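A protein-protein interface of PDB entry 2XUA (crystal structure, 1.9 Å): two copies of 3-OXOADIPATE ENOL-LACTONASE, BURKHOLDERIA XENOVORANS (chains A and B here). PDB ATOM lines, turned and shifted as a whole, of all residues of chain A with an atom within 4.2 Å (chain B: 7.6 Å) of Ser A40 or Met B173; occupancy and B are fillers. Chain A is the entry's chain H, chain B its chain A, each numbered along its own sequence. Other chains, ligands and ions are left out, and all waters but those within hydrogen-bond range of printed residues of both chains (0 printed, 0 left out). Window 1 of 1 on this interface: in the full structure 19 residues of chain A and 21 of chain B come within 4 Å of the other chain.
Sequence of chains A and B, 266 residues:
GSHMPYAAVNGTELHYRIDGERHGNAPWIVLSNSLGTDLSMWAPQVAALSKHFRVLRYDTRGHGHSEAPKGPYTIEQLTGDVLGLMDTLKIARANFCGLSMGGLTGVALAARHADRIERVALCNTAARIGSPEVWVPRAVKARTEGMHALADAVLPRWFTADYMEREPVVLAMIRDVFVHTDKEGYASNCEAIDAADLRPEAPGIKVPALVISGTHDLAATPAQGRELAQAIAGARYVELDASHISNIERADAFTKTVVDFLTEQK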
ATOM      1  N   ASP A  38      15.831  -7.072  25.621  1.00  0.00           N
ATOM      2  CA  ASP A  38      16.675  -7.945  24.839  1.00  0.00           C
ATOM      3  C   ASP A  38      18.115  -7.626  25.181  1.00  0.00           C
ATOM      4  O   ASP A  38      18.375  -6.840  26.084  1.00  0.00           O
ATOM      5  CB  ASP A  38      16.384  -7.824  23.345  1.00  0.00           C
ATOM      6  CG  ASP A  38      16.873  -6.539  22.714  1.00  0.00           C
ATOM      7  OD1 ASP A  38      17.413  -5.687  23.409  1.00  0.00           O
ATOM      8  OD2 ASP A  38      16.731  -6.386  21.474  1.00  0.00           O
ATOM      9  N   LEU A  39      19.068  -8.223  24.449  1.00  0.00           N
ATOM     10  CA  LEU A  39      20.442  -8.110  24.877  1.00  0.00           C
ATOM     11  C   LEU A  39      21.071  -6.725  24.769  1.00  0.00           C
ATOM     12  O   LEU A  39      22.182  -6.534  25.283  1.00  0.00           O
ATOM     13  CB  LEU A  39      21.279  -9.220  24.252  1.00  0.00           C
ATOM     14  CG  LEU A  39      21.922  -9.318  22.852  1.00  0.00           C
ATOM     15  CD1 LEU A  39      21.511 -10.458  22.043  1.00  0.00           C
ATOM     16  CD2 LEU A  39      22.248  -8.061  22.022  1.00  0.00           C
ATOM     17  N   SER A  40      20.379  -5.774  24.112  1.00  0.00           N
ATOM     18  CA  SER A  40      20.823  -4.372  24.067  1.00  0.00           C
ATOM     19  C   SER A  40      20.807  -3.720  25.432  1.00  0.00           C
ATOM     20  O   SER A  40      21.483  -2.682  25.666  1.00  0.00           O
ATOM     21  CB  SER A  40      19.971  -3.539  23.064  1.00  0.00           C
ATOM     22  OG  SER A  40      18.603  -3.340  23.518  1.00  0.00           O
ATOM     23  N   MET A  41      20.032  -4.295  26.363  1.00  0.00           N
ATOM     24  CA  MET A  41      19.949  -3.655  27.707  1.00  0.00           C
ATOM     25  C   MET A  41      21.296  -3.633  28.431  1.00  0.00           C
ATOM     26  O   MET A  41      21.499  -2.810  29.286  1.00  0.00           O
ATOM     27  CB  MET A  41      18.890  -4.326  28.577  1.00  0.00           C
ATOM     28  CG  MET A  41      19.289  -5.762  28.942  1.00  0.00           C
ATOM     29  SD  MET A  41      18.384  -6.229  30.573  1.00  0.00           S
ATOM     30  CE  MET A  41      19.383  -5.189  31.876  1.00  0.00           C
ATOM     31  N   TRP A  42      22.250  -4.508  28.043  1.00  0.00           N
ATOM     32  CA  TRP A  42      23.536  -4.561  28.712  1.00  0.00           C
ATOM     33  C   TRP A  42      24.581  -3.716  27.971  1.00  0.00           C
ATOM     34  O   TRP A  42      25.734  -3.746  28.306  1.00  0.00           O
ATOM     35  CB  TRP A  42      24.033  -6.018  28.693  1.00  0.00           C
ATOM     36  CG  TRP A  42      23.226  -6.896  29.600  1.00  0.00           C
ATOM     37  CD1 TRP A  42      22.425  -7.929  29.230  1.00  0.00           C
ATOM     38  CD2 TRP A  42      23.212  -6.851  31.042  1.00  0.00           C
ATOM     39  NE1 TRP A  42      21.847  -8.493  30.351  1.00  0.00           N
ATOM     40  CE2 TRP A  42      22.320  -7.870  31.478  1.00  0.00           C
ATOM     41  CE3 TRP A  42      23.805  -6.017  31.987  1.00  0.00           C
ATOM     42  CZ2 TRP A  42      22.031  -8.107  32.835  1.00  0.00           C
ATOM     43  CZ3 TRP A  42      23.549  -6.248  33.349  1.00  0.00           C
ATOM     44  CH2 TRP A  42      22.641  -7.292  33.757  1.00  0.00           C
ATOM     45  N   ALA A  43      24.189  -3.020  26.910  1.00  0.00           N
ATOM     46  CA  ALA A  43      25.176  -2.283  26.159  1.00  0.00           C
ATOM     47  C   ALA A  43      26.065  -1.355  27.045  1.00  0.00           C
ATOM     48  O   ALA A  43      27.283  -1.266  26.809  1.00  0.00           O
ATOM     49  CB  ALA A  43      24.459  -1.470  24.966  1.00  0.00           C
ATOM     50  N   MET A 173      13.961   3.727  23.339  1.00  0.00           N
ATOM     51  CA  MET A 173      14.592   2.528  22.798  1.00  0.00           C
ATOM     52  C   MET A 173      14.238   1.288  23.599  1.00  0.00           C
ATOM     53  O   MET A 173      14.011   0.194  23.049  1.00  0.00           O
ATOM     54  CB  MET A 173      16.114   2.748  22.790  1.00  0.00           C
ATOM     55  CG  MET A 173      16.510   3.793  21.669  1.00  0.00           C
ATOM     56  SD  MET A 173      18.434   3.976  21.797  1.00  0.00           S
ATOM     57  CE  MET A 173      19.114   2.559  20.568  1.00  0.00           C
ATOM     58  N   VAL A 177      11.824  -2.098  22.435  1.00  0.00           N
ATOM     59  CA  VAL A 177      12.119  -3.540  22.593  1.00  0.00           C
ATOM     60  C   VAL A 177      10.989  -4.207  23.378  1.00  0.00           C
ATOM     61  O   VAL A 177      10.485  -5.302  23.011  1.00  0.00           O
ATOM     62  CB  VAL A 177      13.444  -3.715  23.363  1.00  0.00           C
ATOM     63  CG1 VAL A 177      13.650  -5.187  23.787  1.00  0.00           C
ATOM     64  CG2 VAL A 177      14.617  -3.189  22.457  1.00  0.00           C
ATOM     65  N   ASP B  38      20.711   0.072  12.802  1.00  0.00           N
ATOM     66  CA  ASP B  38      19.624  -0.786  12.529  1.00  0.00           C
ATOM     67  C   ASP B  38      18.393  -0.025  12.914  1.00  0.00           C
ATOM     68  O   ASP B  38      18.455   1.180  13.204  1.00  0.00           O
ATOM     69  CB  ASP B  38      19.773  -2.158  13.262  1.00  0.00           C
ATOM     70  CG  ASP B  38      19.449  -2.086  14.743  1.00  0.00           C
ATOM     71  OD1 ASP B  38      19.192  -0.969  15.222  1.00  0.00           O
ATOM     72  OD2 ASP B  38      19.527  -3.137  15.485  1.00  0.00           O
ATOM     73  N   SER B  40      16.520   0.241  15.200  1.00  0.00           N
ATOM     74  CA  SER B  40      16.400   0.799  16.571  1.00  0.00           C
ATOM     75  C   SER B  40      16.757   2.274  16.571  1.00  0.00           C
ATOM     76  O   SER B  40      16.324   3.079  17.444  1.00  0.00           O
ATOM     77  CB  SER B  40      17.310   0.030  17.563  1.00  0.00           C
ATOM     78  OG  SER B  40      18.680   0.364  17.415  1.00  0.00           O
ATOM     79  N   GLU B 167      25.491  11.261  27.380  1.00  0.00           N
ATOM     80  CA  GLU B 167      24.569  10.186  27.078  1.00  0.00           C
ATOM     81  C   GLU B 167      25.326   8.862  26.779  1.00  0.00           C
ATOM     82  O   GLU B 167      25.203   8.313  25.643  1.00  0.00           O
ATOM     83  CB  GLU B 167      23.696  10.550  25.887  1.00  0.00           C
ATOM     84  CG  GLU B 167      22.788  11.828  26.069  1.00  0.00           C
ATOM     85  CD  GLU B 167      21.698  11.613  27.084  1.00  0.00           C
ATOM     86  OE1 GLU B 167      21.109  12.615  27.547  1.00  0.00           O
ATOM     87  OE2 GLU B 167      21.426  10.418  27.434  1.00  0.00           O
ATOM     88  N   PRO B 168      26.112   8.360  27.756  1.00  0.00           N
ATOM     89  CA  PRO B 168      26.919   7.182  27.492  1.00  0.00           C
ATOM     90  C   PRO B 168      26.036   5.895  27.245  1.00  0.00           C
ATOM     91  O   PRO B 168      26.526   4.960  26.603  1.00  0.00           O
ATOM     92  CB  PRO B 168      27.651   6.958  28.807  1.00  0.00           C
ATOM     93  CG  PRO B 168      26.732   7.711  29.897  1.00  0.00           C
ATOM     94  CD  PRO B 168      26.294   8.880  29.119  1.00  0.00           C
ATOM     95  N   VAL B 169      24.789   5.861  27.741  1.00  0.00           N
ATOM     96  CA  VAL B 169      23.940   4.639  27.517  1.00  0.00           C
ATOM     97  C   VAL B 169      23.488   4.662  26.037  1.00  0.00           C
ATOM     98  O   VAL B 169      23.596   3.646  25.334  1.00  0.00           O
ATOM     99  CB  VAL B 169      22.706   4.612  28.464  1.00  0.00           C
ATOM    100  CG1 VAL B 169      21.631   3.529  28.036  1.00  0.00           C
ATOM    101  CG2 VAL B 169      23.162   4.403  30.021  1.00  0.00           C
ATOM    102  N   VAL B 170      22.994   5.821  25.578  1.00  0.00           N
ATOM    103  CA  VAL B 170      22.595   5.957  24.134  1.00  0.00           C
ATOM    104  C   VAL B 170      23.824   5.629  23.279  1.00  0.00           C
ATOM    105  O   VAL B 170      23.767   4.834  22.329  1.00  0.00           O
ATOM    106  CB  VAL B 170      22.052   7.378  23.784  1.00  0.00           C
ATOM    107  CG1 VAL B 170      21.770   7.486  22.278  1.00  0.00           C
ATOM    108  CG2 VAL B 170      20.707   7.717  24.591  1.00  0.00           C
ATOM    109  N   LEU B 171      24.959   6.250  23.594  1.00  0.00           N
ATOM    110  CA  LEU B 171      26.133   5.979  22.774  1.00  0.00           C
ATOM    111  C   LEU B 171      26.474   4.469  22.781  1.00  0.00           C
ATOM    112  O   LEU B 171      26.751   3.842  21.707  1.00  0.00           O
ATOM    113  CB  LEU B 171      27.297   6.756  23.306  1.00  0.00           C
ATOM    114  CG  LEU B 171      28.189   7.510  22.348  1.00  0.00           C
ATOM    115  CD1 LEU B 171      29.528   7.793  23.190  1.00  0.00           C
ATOM    116  CD2 LEU B 171      28.558   6.798  20.986  1.00  0.00           C
ATOM    117  N   ALA B 172      26.480   3.875  23.975  1.00  0.00           N
ATOM    118  CA  ALA B 172      26.793   2.440  24.069  1.00  0.00           C
ATOM    119  C   ALA B 172      25.826   1.577  23.279  1.00  0.00           C
ATOM    120  O   ALA B 172      26.244   0.577  22.694  1.00  0.00           O
ATOM    121  CB  ALA B 172      26.853   1.971  25.503  1.00  0.00           C
ATOM    122  N   MET B 173      24.535   1.921  23.301  1.00  0.00           N
ATOM    123  CA  MET B 173      23.583   1.176  22.501  1.00  0.00           C
ATOM    124  C   MET B 173      23.818   1.293  21.005  1.00  0.00           C
ATOM    125  O   MET B 173      23.757   0.276  20.273  1.00  0.00           O
ATOM    126  CB  MET B 173      22.153   1.572  22.832  1.00  0.00           C
ATOM    127  CG  MET B 173      21.764   0.903  24.116  1.00  0.00           C
ATOM    128  SD  MET B 173      20.131   1.676  24.768  1.00  0.00           S
ATOM    129  CE  MET B 173      18.877   0.321  24.113  1.00  0.00           C
ATOM    130  N   ILE B 174      24.075   2.517  20.552  1.00  0.00           N
ATOM    131  CA  ILE B 174      24.278   2.764  19.150  1.00  0.00           C
ATOM    132  C   ILE B 174      25.572   2.106  18.714  1.00  0.00           C
ATOM    133  O   ILE B 174      25.641   1.522  17.631  1.00  0.00           O
ATOM    134  CB  ILE B 174      24.302   4.334  18.853  1.00  0.00           C
ATOM    135  CG1 ILE B 174      22.892   4.861  19.056  1.00  0.00           C
ATOM    136  CG2 ILE B 174      24.764   4.633  17.394  1.00  0.00           C
ATOM    137  CD1 ILE B 174      21.792   4.125  18.170  1.00  0.00           C
ATOM    138  N   ARG B 175      26.606   2.213  19.558  1.00  0.00           N
ATOM    139  CA  ARG B 175      27.911   1.682  19.260  1.00  0.00           C
ATOM    140  C   ARG B 175      27.766   0.136  19.157  1.00  0.00           C
ATOM    141  O   ARG B 175      28.382  -0.471  18.286  1.00  0.00           O
ATOM    142  CB  ARG B 175      28.901   2.016  20.356  1.00  0.00           C
ATOM    143  CG  ARG B 175      30.281   1.371  20.146  1.00  0.00           C
ATOM    144  CD  ARG B 175      31.377   1.905  21.091  1.00  0.00           C
ATOM    145  NE  ARG B 175      32.588   1.105  20.870  1.00  0.00           N
ATOM    146  CZ  ARG B 175      33.698   1.532  20.273  1.00  0.00           C
ATOM    147  NH1 ARG B 175      33.840   2.816  19.864  1.00  0.00           N
ATOM    148  NH2 ARG B 175      34.699   0.671  20.110  1.00  0.00           N
ATOM    149  N   ASP B 176      26.987  -0.456  20.065  1.00  0.00           N
ATOM    150  CA  ASP B 176      26.843  -1.948  20.033  1.00  0.00           C
ATOM    151  C   ASP B 176      26.284  -2.397  18.682  1.00  0.00           C
ATOM    152  O   ASP B 176      26.785  -3.385  18.120  1.00  0.00           O
ATOM    153  CB  ASP B 176      25.896  -2.446  21.138  1.00  0.00           C
ATOM    154  CG  ASP B 176      25.968  -3.951  21.317  1.00  0.00           C
ATOM    155  OD1 ASP B 176      27.105  -4.479  21.353  1.00  0.00           O
ATOM    156  OD2 ASP B 176      24.897  -4.596  21.487  1.00  0.00           O
ATOM    157  N   VAL B 177      25.252  -1.695  18.157  1.00  0.00           N
ATOM    158  CA  VAL B 177      24.670  -2.079  16.837  1.00  0.00           C
ATOM    159  C   VAL B 177      25.741  -1.920  15.714  1.00  0.00           C
ATOM    160  O   VAL B 177      25.844  -2.781  14.851  1.00  0.00           O
ATOM    161  CB  VAL B 177      23.420  -1.301  16.492  1.00  0.00           C
ATOM    162  CG1 VAL B 177      23.052  -1.461  14.937  1.00  0.00           C
ATOM    163  CG2 VAL B 177      22.244  -1.656  17.502  1.00  0.00           C
ATOM    164  N   PHE B 178      26.524  -0.828  15.760  1.00  0.00           N
ATOM    165  CA  PHE B 178      27.546  -0.552  14.744  1.00  0.00           C
ATOM    166  C   PHE B 178      28.608  -1.663  14.722  1.00  0.00           C
ATOM    167  O   PHE B 178      29.013  -2.230  13.683  1.00  0.00           O
ATOM    168  CB  PHE B 178      28.205   0.828  15.054  1.00  0.00           C
ATOM    169  CG  PHE B 178      29.254   1.198  14.066  1.00  0.00           C
ATOM    170  CD1 PHE B 178      28.938   1.966  12.968  1.00  0.00           C
ATOM    171  CD2 PHE B 178      30.581   0.739  14.229  1.00  0.00           C
ATOM    172  CE1 PHE B 178      29.962   2.323  12.023  1.00  0.00           C
ATOM    173  CE2 PHE B 178      31.567   1.045  13.300  1.00  0.00           C
ATOM    174  CZ  PHE B 178      31.257   1.817  12.203  1.00  0.00           C
ATOM    175  N   VAL B 179      29.055  -2.001  15.902  1.00  0.00           N
ATOM    176  CA  VAL B 179      30.207  -2.890  16.052  1.00  0.00           C
ATOM    177  C   VAL B 179      29.787  -4.364  15.723  1.00  0.00           C
ATOM    178  O   VAL B 179      30.611  -5.242  15.353  1.00  0.00           O
ATOM    179  CB  VAL B 179      30.783  -2.520  17.486  1.00  0.00           C
ATOM    180  CG1 VAL B 179      30.720  -3.577  18.514  1.00  0.00           C
ATOM    181  CG2 VAL B 179      32.050  -1.621  17.397  1.00  0.00           C
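The side-chain carboxylate (OD1) of Asp B38 is in hydrogen-bond range of the side-chain hydroxyl (OG) of Ser B40 (2.6 Å). The side-chain carboxylate of Asp A38 is in hydrogen-bond range of the side-chain hydroxyl of Ser A40.
Among the printed residues, pairs that only touch across the chains: Ser A40 with Met B173, Ala A43 with Ala B172, Ala A43 with Met B173, Met A173 with Ser B40, Met A173 with Met B173 and Met A173 with Ile B174.
Met B173 touches just these residues of chain A: Ser A40, Ala A43 and Met A173. Of the printed residues of chain A, Ala B172 touches Ala A43 (3.5 Å). Printed residues of chain B within 4 Å of Ala A43: Ala B172 and Met B173. Of the printed residues of chain A, Ile B174 touches Met A173 (3.9 Å). The nearest residue of chain B that does not touch Ser A40 is Asp B176 (4.8 Å). The nearest printed residue of chain A that does not touch Met B173 is Met A41 (5.3 Å). The nearest printed residue of chain B that does not touch Ala A43 is Asp B176 (4.2 Å).
Of the 15 printed residues of chain B, 4 touch a printed residue of chain A. Hydrophobic or aromatic side chains of chain B within 4 Å of the printed part of chain A: Ala B172, Met B173 and Ile B174. Hydrophobic or aromatic side chains of chain A within 4 Å of the printed part of chain B: Ala A43 and Met A173. Among the printed residues, 6 pairs touch across the chains.
Ser A40 touches Met B173, and with the chains exchanged Met A173 touches Ser B40. Met B173 touches its own counterpart, Met A173. Positions printed for both chains: 38, 40, 173 and 177.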
